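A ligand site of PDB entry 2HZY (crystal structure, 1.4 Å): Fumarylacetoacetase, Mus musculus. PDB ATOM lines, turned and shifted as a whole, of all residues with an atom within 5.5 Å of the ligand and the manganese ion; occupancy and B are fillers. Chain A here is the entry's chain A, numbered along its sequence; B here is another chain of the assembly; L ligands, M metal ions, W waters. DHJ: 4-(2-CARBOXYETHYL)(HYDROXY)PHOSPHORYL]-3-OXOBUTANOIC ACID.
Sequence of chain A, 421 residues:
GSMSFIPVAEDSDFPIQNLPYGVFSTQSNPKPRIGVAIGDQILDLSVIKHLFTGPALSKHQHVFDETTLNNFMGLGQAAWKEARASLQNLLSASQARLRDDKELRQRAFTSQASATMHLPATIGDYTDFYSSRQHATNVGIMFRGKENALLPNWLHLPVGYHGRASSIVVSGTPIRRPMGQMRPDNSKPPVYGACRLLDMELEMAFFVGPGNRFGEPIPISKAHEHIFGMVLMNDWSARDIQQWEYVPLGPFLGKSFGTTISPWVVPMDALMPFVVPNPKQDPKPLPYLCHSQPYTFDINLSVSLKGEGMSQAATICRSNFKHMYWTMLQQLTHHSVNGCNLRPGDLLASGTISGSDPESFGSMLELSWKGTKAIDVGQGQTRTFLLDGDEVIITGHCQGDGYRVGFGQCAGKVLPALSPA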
ATOM      1  N   TYR A 126      15.544  15.600  37.626  1.00  0.00           N
ATOM      2  CA  TYR A 126      14.787  14.477  37.091  1.00  0.00           C
ATOM      3  C   TYR A 126      14.576  14.736  35.633  1.00  0.00           C
ATOM      4  O   TYR A 126      14.198  15.833  35.198  1.00  0.00           O
ATOM      5  CB  TYR A 126      13.457  14.369  37.887  1.00  0.00           C
ATOM      6  CG  TYR A 126      12.278  13.722  37.181  1.00  0.00           C
ATOM      7  CD1 TYR A 126      11.059  14.379  37.136  1.00  0.00           C
ATOM      8  CD2 TYR A 126      12.406  12.489  36.547  1.00  0.00           C
ATOM      9  CE1 TYR A 126       9.966  13.800  36.466  1.00  0.00           C
ATOM     10  CE2 TYR A 126      11.357  11.936  35.856  1.00  0.00           C
ATOM     11  CZ  TYR A 126      10.141  12.596  35.856  1.00  0.00           C
ATOM     12  OH  TYR A 126       9.104  12.102  35.079  1.00  0.00           O
ATOM     13  N   ASP A 128      12.685  12.852  32.132  1.00  0.00           N
ATOM     14  CA  ASP A 128      11.796  11.779  31.643  1.00  0.00           C
ATOM     15  C   ASP A 128      12.100  11.596  30.154  1.00  0.00           C
ATOM     16  O   ASP A 128      11.981  12.524  29.348  1.00  0.00           O
ATOM     17  CB  ASP A 128      10.341  12.145  31.891  1.00  0.00           C
ATOM     18  CG  ASP A 128       9.371  11.029  31.638  1.00  0.00           C
ATOM     19  OD1 ASP A 128       9.824   9.858  31.795  1.00  0.00           O
ATOM     20  OD2 ASP A 128       8.178  11.253  31.341  1.00  0.00           O
ATOM     21  N   PHE A 129      12.489  10.377  29.795  1.00  0.00           N
ATOM     22  CA  PHE A 129      12.682  10.022  28.378  1.00  0.00           C
ATOM     23  C   PHE A 129      11.369   9.563  27.755  1.00  0.00           C
ATOM     24  O   PHE A 129      10.288   9.677  28.348  1.00  0.00           O
ATOM     25  CB  PHE A 129      13.857   9.015  28.257  1.00  0.00           C
ATOM     26  CG  PHE A 129      15.198   9.660  28.493  1.00  0.00           C
ATOM     27  CD1 PHE A 129      15.800   9.704  29.748  1.00  0.00           C
ATOM     28  CD2 PHE A 129      15.826  10.289  27.408  1.00  0.00           C
ATOM     29  CE1 PHE A 129      16.997  10.356  29.936  1.00  0.00           C
ATOM     30  CE2 PHE A 129      17.047  10.921  27.585  1.00  0.00           C
ATOM     31  CZ  PHE A 129      17.636  10.949  28.831  1.00  0.00           C
ATOM     32  N   TYR A 130      11.449   9.068  26.522  1.00  0.00           N
ATOM     33  CA  TYR A 130      10.275   8.823  25.694  1.00  0.00           C
ATOM     34  C   TYR A 130      10.597   7.610  24.826  1.00  0.00           C
ATOM     35  O   TYR A 130      10.288   7.564  23.619  1.00  0.00           O
ATOM     36  CB  TYR A 130      10.041  10.098  24.857  1.00  0.00           C
ATOM     37  CG  TYR A 130       8.831  10.240  23.990  1.00  0.00           C
ATOM     38  CD1 TYR A 130       7.578   9.798  24.396  1.00  0.00           C
ATOM     39  CD2 TYR A 130       8.920  10.902  22.778  1.00  0.00           C
ATOM     40  CE1 TYR A 130       6.456  10.027  23.649  1.00  0.00           C
ATOM     41  CE2 TYR A 130       7.815  11.116  22.031  1.00  0.00           C
ATOM     42  CZ  TYR A 130       6.600  10.692  22.442  1.00  0.00           C
ATOM     43  OH  TYR A 130       5.383  10.861  21.758  1.00  0.00           O
ATOM     44  N   SER A 131      11.179   6.594  25.467  1.00  0.00           N
ATOM     45  CA  SER A 131      11.943   5.589  24.695  1.00  0.00           C
ATOM     46  C   SER A 131      11.187   4.319  24.273  1.00  0.00           C
ATOM     47  O   SER A 131      11.831   3.428  23.705  1.00  0.00           O
ATOM     48  CB  SER A 131      13.250   5.220  25.412  1.00  0.00           C
ATOM     49  OG  SER A 131      14.084   6.390  25.580  1.00  0.00           O
ATOM     50  N   HIS A 135       4.726   3.406  22.651  1.00  0.00           N
ATOM     51  CA  HIS A 135       4.120   4.534  23.313  1.00  0.00           C
ATOM     52  C   HIS A 135       4.181   5.795  22.476  1.00  0.00           C
ATOM     53  O   HIS A 135       3.186   6.480  22.339  1.00  0.00           O
ATOM     54  CB  HIS A 135       4.766   4.780  24.683  1.00  0.00           C
ATOM     55  CG  HIS A 135       4.295   6.030  25.348  1.00  0.00           C
ATOM     56  ND1 HIS A 135       3.070   6.166  25.985  1.00  0.00           N
ATOM     57  CD2 HIS A 135       4.931   7.218  25.500  1.00  0.00           C
ATOM     58  CE1 HIS A 135       2.956   7.409  26.440  1.00  0.00           C
ATOM     59  NE2 HIS A 135       4.069   8.076  26.149  1.00  0.00           N
ATOM     60  N   ALA A 136       5.381   6.137  21.987  1.00  0.00           N
ATOM     61  CA  ALA A 136       5.498   7.299  21.110  1.00  0.00           C
ATOM     62  C   ALA A 136       4.629   7.204  19.850  1.00  0.00           C
ATOM     63  O   ALA A 136       4.044   8.208  19.478  1.00  0.00           O
ATOM     64  CB  ALA A 136       6.999   7.528  20.732  1.00  0.00           C
ATOM     65  N   VAL A 139       0.880   7.752  20.979  1.00  0.00           N
ATOM     66  CA  VAL A 139       0.604   9.152  21.225  1.00  0.00           C
ATOM     67  C   VAL A 139       0.517   9.805  19.807  1.00  0.00           C
ATOM     68  O   VAL A 139      -0.446  10.522  19.482  1.00  0.00           O
ATOM     69  CB  VAL A 139       1.566   9.793  22.262  1.00  0.00           C
ATOM     70  CG1 VAL A 139       1.267  11.265  22.439  1.00  0.00           C
ATOM     71  CG2 VAL A 139       1.416   9.112  23.637  1.00  0.00           C
ATOM     72  N   GLY A 140       1.473   9.461  18.936  1.00  0.00           N
ATOM     73  CA  GLY A 140       1.452   9.996  17.583  1.00  0.00           C
ATOM     74  C   GLY A 140       0.195   9.656  16.798  1.00  0.00           C
ATOM     75  O   GLY A 140      -0.354  10.544  16.089  1.00  0.00           O
ATOM     76  N   PHE A 143      -2.743  11.719  18.175  1.00  0.00           N
ATOM     77  CA  PHE A 143      -2.651  13.177  18.149  1.00  0.00           C
ATOM     78  C   PHE A 143      -2.359  13.784  16.756  1.00  0.00           C
ATOM     79  O   PHE A 143      -2.700  14.931  16.490  1.00  0.00           O
ATOM     80  CB  PHE A 143      -1.463  13.601  19.021  1.00  0.00           C
ATOM     81  CG  PHE A 143      -1.737  13.716  20.474  1.00  0.00           C
ATOM     82  CD1 PHE A 143      -0.877  14.524  21.234  1.00  0.00           C
ATOM     83  CD2 PHE A 143      -2.762  13.021  21.107  1.00  0.00           C
ATOM     84  CE1 PHE A 143      -1.071  14.659  22.617  1.00  0.00           C
ATOM     85  CE2 PHE A 143      -2.983  13.152  22.503  1.00  0.00           C
ATOM     86  CZ  PHE A 143      -2.132  13.971  23.244  1.00  0.00           C
ATOM     87  N   ARG A 144      -1.673  13.017  15.914  1.00  0.00           N
ATOM     88  CA  ARG A 144      -1.065  13.587  14.738  1.00  0.00           C
ATOM     89  C   ARG A 144      -1.429  12.675  13.531  1.00  0.00           C
ATOM     90  O   ARG A 144      -1.243  13.058  12.359  1.00  0.00           O
ATOM     91  CB  ARG A 144       0.489  13.764  14.947  1.00  0.00           C
ATOM     92  CG  ARG A 144       0.953  14.763  16.189  1.00  0.00           C
ATOM     93  CD  ARG A 144       2.498  14.694  16.683  1.00  0.00           C
ATOM     94  NE  ARG A 144       2.661  15.344  18.016  1.00  0.00           N
ATOM     95  CZ  ARG A 144       3.089  14.787  19.189  1.00  0.00           C
ATOM     96  NH1 ARG A 144       3.554  13.544  19.280  1.00  0.00           N
ATOM     97  NH2 ARG A 144       3.022  15.539  20.308  1.00  0.00           N
ATOM     98  N   TYR A 161      12.747  15.126  28.266  1.00  0.00           N
ATOM     99  CA  TYR A 161      12.553  16.519  28.739  1.00  0.00           C
ATOM    100  C   TYR A 161      12.887  16.544  30.210  1.00  0.00           C
ATOM    101  O   TYR A 161      12.878  15.495  30.915  1.00  0.00           O
ATOM    102  CB  TYR A 161      11.097  17.000  28.491  1.00  0.00           C
ATOM    103  CG  TYR A 161      10.054  16.219  29.276  1.00  0.00           C
ATOM    104  CD1 TYR A 161       9.456  16.773  30.418  1.00  0.00           C
ATOM    105  CD2 TYR A 161       9.688  14.931  28.879  1.00  0.00           C
ATOM    106  CE1 TYR A 161       8.552  16.027  31.199  1.00  0.00           C
ATOM    107  CE2 TYR A 161       8.745  14.180  29.647  1.00  0.00           C
ATOM    108  CZ  TYR A 161       8.195  14.757  30.790  1.00  0.00           C
ATOM    109  OH  TYR A 161       7.336  14.011  31.572  1.00  0.00           O
ATOM    110  N   GLU A 201       1.149   6.856  34.162  1.00  0.00           N
ATOM    111  CA  GLU A 201       2.102   6.404  33.154  1.00  0.00           C
ATOM    112  C   GLU A 201       3.030   5.421  33.793  1.00  0.00           C
ATOM    113  O   GLU A 201       3.793   5.765  34.705  1.00  0.00           O
ATOM    114  CB  GLU A 201       2.955   7.545  32.584  1.00  0.00           C
ATOM    115  CG  GLU A 201       2.193   8.491  31.639  1.00  0.00           C
ATOM    116  CD  GLU A 201       3.162   9.422  30.885  1.00  0.00           C
ATOM    117  OE1 GLU A 201       2.859   9.830  29.750  1.00  0.00           O
ATOM    118  OE2 GLU A 201       4.226   9.740  31.379  1.00  0.00           O
ATOM    119  N   GLU A 203       6.296   3.685  34.164  1.00  0.00           N
ATOM    120  CA  GLU A 203       7.699   3.893  33.762  1.00  0.00           C
ATOM    121  C   GLU A 203       8.605   3.172  34.726  1.00  0.00           C
ATOM    122  O   GLU A 203       8.182   2.718  35.787  1.00  0.00           O
ATOM    123  CB  GLU A 203       8.039   5.407  33.780  1.00  0.00           C
ATOM    124  CG  GLU A 203       7.045   6.217  32.942  1.00  0.00           C
ATOM    125  CD  GLU A 203       7.550   7.574  32.525  1.00  0.00           C
ATOM    126  OE1 GLU A 203       8.775   7.691  32.250  1.00  0.00           O
ATOM    127  OE2 GLU A 203       6.735   8.528  32.444  1.00  0.00           O
ATOM    128  N   ASP A 235       4.335   8.377  36.278  1.00  0.00           N
ATOM    129  CA  ASP A 235       4.370   9.781  35.889  1.00  0.00           C
ATOM    130  C   ASP A 235       2.926  10.263  35.720  1.00  0.00           C
ATOM    131  O   ASP A 235       2.432  10.358  34.598  1.00  0.00           O
ATOM    132  CB  ASP A 235       5.216   9.936  34.602  1.00  0.00           C
ATOM    133  CG  ASP A 235       5.380  11.350  34.143  1.00  0.00           C
ATOM    134  OD1 ASP A 235       5.109  12.306  34.946  1.00  0.00           O
ATOM    135  OD2 ASP A 235       5.781  11.552  32.934  1.00  0.00           O
ATOM    136  N   SER A 237      -0.239  12.295  34.988  1.00  0.00           N
ATOM    137  CA  SER A 237      -0.350  13.248  33.865  1.00  0.00           C
ATOM    138  C   SER A 237      -1.769  13.794  33.824  1.00  0.00           C
ATOM    139  O   SER A 237      -2.748  13.060  34.052  1.00  0.00           O
ATOM    140  CB  SER A 237      -0.007  12.553  32.526  1.00  0.00           C
ATOM    141  OG  SER A 237       1.315  12.008  32.605  1.00  0.00           O
ATOM    142  N   ARG A 239      -3.976  15.204  31.073  1.00  0.00           N
ATOM    143  CA  ARG A 239      -3.790  15.228  29.611  1.00  0.00           C
ATOM    144  C   ARG A 239      -4.396  16.464  28.953  1.00  0.00           C
ATOM    145  O   ARG A 239      -3.920  16.905  27.914  1.00  0.00           O
ATOM    146  CB  ARG A 239      -4.345  13.972  28.944  1.00  0.00           C
ATOM    147  CG  ARG A 239      -3.689  12.679  29.400  1.00  0.00           C
ATOM    148  CD  ARG A 239      -2.188  12.660  29.231  1.00  0.00           C
ATOM    149  NE  ARG A 239      -1.640  11.308  29.395  1.00  0.00           N
ATOM    150  CZ  ARG A 239      -0.380  11.007  29.137  1.00  0.00           C
ATOM    151  NH1 ARG A 239       0.468  11.936  28.700  1.00  0.00           N
ATOM    152  NH2 ARG A 239       0.048   9.762  29.261  1.00  0.00           N
ATOM    153  N   GLN A 242      -1.973  19.231  29.724  1.00  0.00           N
ATOM    154  CA  GLN A 242      -0.824  18.976  28.882  1.00  0.00           C
ATOM    155  C   GLN A 242      -1.026  19.416  27.447  1.00  0.00           C
ATOM    156  O   GLN A 242      -0.173  20.105  26.872  1.00  0.00           O
ATOM    157  CB  GLN A 242      -0.473  17.488  28.955  1.00  0.00           C
ATOM    158  CG  GLN A 242       0.821  17.111  28.221  1.00  0.00           C
ATOM    159  CD  GLN A 242       1.176  15.636  28.355  1.00  0.00           C
ATOM    160  OE1 GLN A 242       0.595  14.911  29.200  1.00  0.00           O
ATOM    161  NE2 GLN A 242       2.095  15.169  27.550  1.00  0.00           N
ATOM    162  N   TYR A 246       1.544  22.506  25.842  1.00  0.00           N
ATOM    163  CA  TYR A 246       2.866  21.928  25.593  1.00  0.00           C
ATOM    164  C   TYR A 246       3.560  22.439  24.354  1.00  0.00           C
ATOM    165  O   TYR A 246       4.744  22.152  24.179  1.00  0.00           O
ATOM    166  CB  TYR A 246       2.843  20.371  25.604  1.00  0.00           C
ATOM    167  CG  TYR A 246       2.475  19.752  24.290  1.00  0.00           C
ATOM    168  CD1 TYR A 246       3.464  19.201  23.454  1.00  0.00           C
ATOM    169  CD2 TYR A 246       1.167  19.743  23.857  1.00  0.00           C
ATOM    170  CE1 TYR A 246       3.123  18.649  22.204  1.00  0.00           C
ATOM    171  CE2 TYR A 246       0.807  19.190  22.624  1.00  0.00           C
ATOM    172  CZ  TYR A 246       1.774  18.632  21.823  1.00  0.00           C
ATOM    173  OH  TYR A 246       1.401  18.085  20.588  1.00  0.00           O
ATOM    174  N   PRO A 251       5.923  19.391  27.871  1.00  0.00           N
ATOM    175  CA  PRO A 251       4.983  19.181  28.993  1.00  0.00           C
ATOM    176  C   PRO A 251       5.492  19.896  30.236  1.00  0.00           C
ATOM    177  O   PRO A 251       6.714  19.969  30.481  1.00  0.00           O
ATOM    178  CB  PRO A 251       5.013  17.666  29.197  1.00  0.00           C
ATOM    179  CG  PRO A 251       6.093  17.114  28.364  1.00  0.00           C
ATOM    180  CD  PRO A 251       6.596  18.167  27.447  1.00  0.00           C
ATOM    181  N   LYS A 255       2.475  17.545  33.966  1.00  0.00           N
ATOM    182  CA  LYS A 255       3.256  16.482  34.591  1.00  0.00           C
ATOM    183  C   LYS A 255       3.657  16.801  36.006  1.00  0.00           C
ATOM    184  O   LYS A 255       3.947  15.850  36.785  1.00  0.00           O
ATOM    185  CB  LYS A 255       4.592  16.271  33.816  1.00  0.00           C
ATOM    186  CG  LYS A 255       4.405  15.867  32.387  1.00  0.00           C
ATOM    187  CD  LYS A 255       3.779  14.507  32.265  1.00  0.00           C
ATOM    188  CE  LYS A 255       3.870  14.034  30.846  1.00  0.00           C
ATOM    189  NZ  LYS A 255       3.324  12.629  30.742  1.00  0.00           N
ATOM    190  N   GLY A 351      10.587   6.671  30.123  1.00  0.00           N
ATOM    191  CA  GLY A 351       9.416   6.855  29.259  1.00  0.00           C
ATOM    192  C   GLY A 351       8.349   5.814  29.608  1.00  0.00           C
ATOM    193  O   GLY A 351       8.617   4.780  30.242  1.00  0.00           O
ATOM    194  N   THR A 352       7.122   6.082  29.184  1.00  0.00           N
ATOM    195  CA  THR A 352       6.021   5.147  29.374  1.00  0.00           C
ATOM    196  C   THR A 352       6.283   3.868  28.630  1.00  0.00           C
ATOM    197  O   THR A 352       6.620   3.858  27.418  1.00  0.00           O
ATOM    198  CB  THR A 352       4.729   5.831  28.924  1.00  0.00           C
ATOM    199  OG1 THR A 352       4.533   6.994  29.733  1.00  0.00           O
ATOM    200  CG2 THR A 352       3.494   4.911  29.114  1.00  0.00           C
ATOM    201  N   PRO B 248       8.607  16.662  20.172  1.00  0.00           N
ATOM    202  CA  PRO B 248       7.558  17.509  20.754  1.00  0.00           C
ATOM    203  C   PRO B 248       7.778  17.860  22.240  1.00  0.00           C
ATOM    204  O   PRO B 248       6.866  18.494  22.809  1.00  0.00           O
ATOM    205  CB  PRO B 248       6.347  16.563  20.636  1.00  0.00           C
ATOM    206  CG  PRO B 248       6.899  15.165  20.862  1.00  0.00           C
ATOM    207  CD  PRO B 248       8.357  15.229  20.414  1.00  0.00           C
ATOM    208  N   LEU B 249       8.869  17.461  22.865  1.00  0.00           N
ATOM    209  CA  LEU B 249       8.945  17.566  24.323  1.00  0.00           C
ATOM    210  C   LEU B 249       9.736  18.744  24.833  1.00  0.00           C
ATOM    211  O   LEU B 249       9.849  18.903  26.068  1.00  0.00           O
ATOM    212  CB  LEU B 249       9.479  16.263  24.971  1.00  0.00           C
ATOM    213  CG  LEU B 249       8.610  15.031  24.586  1.00  0.00           C
ATOM    214  CD1 LEU B 249       9.091  13.776  25.313  1.00  0.00           C
ATOM    215  CD2 LEU B 249       7.058  15.229  24.759  1.00  0.00           C
HETATM  216  O2  DHJ L   1       3.462  14.723  23.113  1.00  0.00           O
HETATM  217  C3  DHJ L   1       3.960  13.537  23.014  1.00  0.00           C
HETATM  218  O4  DHJ L   1       4.276  13.082  21.926  1.00  0.00           O
HETATM  219  C1  DHJ L   1       4.203  12.625  24.199  1.00  0.00           C
HETATM  220  C7  DHJ L   1       3.925  13.018  25.451  1.00  0.00           C
HETATM  221  P1  DHJ L   1       4.182  12.058  26.897  1.00  0.00           P
HETATM  222  O6  DHJ L   1       3.097  12.476  27.868  1.00  0.00           O
HETATM  223  O7  DHJ L   1       4.373  10.595  26.638  1.00  0.00           O
HETATM  224  C6  DHJ L   1       5.762  12.688  27.544  1.00  0.00           C
HETATM  225  C5  DHJ L   1       6.274  11.767  28.593  1.00  0.00           C
HETATM  226  O5  DHJ L   1       5.892  11.771  29.779  1.00  0.00           O
HETATM  227  C4  DHJ L   1       7.346  10.749  28.176  1.00  0.00           C
HETATM  228  C2  DHJ L   1       6.929   9.309  28.490  1.00  0.00           C
HETATM  229  O1  DHJ L   1       6.516   9.043  29.651  1.00  0.00           O
HETATM  230  O3  DHJ L   1       7.029   8.440  27.570  1.00  0.00           O
HETATM  231 MN    MN M   1       6.271  10.259  31.329  1.00  0.00          MN
HETATM  232  O   HOH W   1       2.816  16.514  25.219  1.00  0.00           O
HETATM  233  O   HOH W   2       7.993   6.002  26.104  1.00  0.00           O
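The side-chain hydroxyl (OH) of Tyr 161 sits close to an oxygen (O5) of the ligand (3.2 Å).
NH1 of Arg 144 lies within salt-bridge range of O4 of the ligand (2.8 Å).
O6 of the ligand lies within salt-bridge range of NZ of Lys 255 (2.9 Å).
A ring nitrogen (NE2) of His 135 is in hydrogen-bond range of an oxygen (O7) of the ligand, at 2.6 Å.
An oxygen (O1) of the ligand lies close to the side-chain hydroxyl (OG1) of Thr 352.
An oxygen (O4) of the ligand sits at hydrogen-bond distance from the side-chain hydroxyl of Tyr 130 (2.5 Å).
The side-chain amide nitrogen of Gln 242 is in hydrogen-bond range of an oxygen (O6) of the ligand (2.9 Å).
NH1 of Arg 239 lies within salt-bridge range of O6 of the ligand.
N of Thr 352 sits at hydrogen-bond distance from O3 of the ligand.
The side-chain hydroxyl (OH) of Tyr 161 lies close to the side-chain carboxylate (OD2) of Asp 235, 3.2 Å away.
The side-chain amino group (NZ) of Lys 255 sits close to the side-chain carboxylate (OD2) of Asp 235 (3.5 Å).
The side-chain carboxylate (OE1) of Glu 201 is in salt-bridge range of the side-chain amino group (NZ) of Lys 255 (3.0 Å).
The side-chain carboxylate (OE1) of Glu 201 lies close to the side-chain hydroxyl (OG1) of Thr 352.
The side-chain hydroxyl of Ser 237 lies within hydrogen-bond range of the side-chain amino group of Lys 255 (2.8 Å).
The guanidinium group (NH2) of Arg 144 lies within hydrogen-bond range of the side-chain hydroxyl (OH) of Tyr 246, 3.0 Å away.
N of Asp 128 is in hydrogen-bond range of O of Tyr 161 (2.9 Å).
OE1 of Gln 242 is in hydrogen-bond range of NH1 of Arg 239 (3.0 Å).
Phe 129 touches the ligand.
CG1 of Val 139 touches O4 of the ligand, 3.6 Å away.
Gly 351 touches the ligand.
Pro 248 of chain B touches the ligand (CG to O4, 3.5 Å).
Leu 249 of chain B touches the ligand (CD2 to C7, 3.9 Å).
Hydrophobic or aromatic side chains that line the ligand: Tyr 130, His 135, Val 139, Tyr 161, Pro 248 of chain B and Leu 249 of chain B.
Of the 25 residues printed, 17 come within 4 Å of the ligand.
The nearest printed residue that does not touch the ligand is Tyr 246 (4.04 Å).
Tyr 161 touches the manganese ion.
Lys 255 touches the manganese ion.
Six residues have an atom within 4 Å of the manganese ion: Asp 128, Tyr 161, Glu 201, Glu 203, Asp 235 and Lys 255.
O1 of the ligand binds the manganese ion, 2.1 Å away.
The manganese ion is bound by OE2 of Glu 201, 2.1 Å away.
The side-chain carboxylate (OE2) of Glu 203 is bound to the manganese ion, 2.1 Å away.
OD2 of Asp 235 is bound to the manganese ion, at 2.1 Å.
OD2 of Asp 128 is bound to the manganese ion (2.2 Å).
O5 of the ligand binds the manganese ion (2.2 Å).
Water W1 bridges NE2 of Gln 242 and O2 of the ligand.
Water W2 lies within hydrogen-bond range of O of Thr 352, O3 of the ligand and N of Ser 131.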
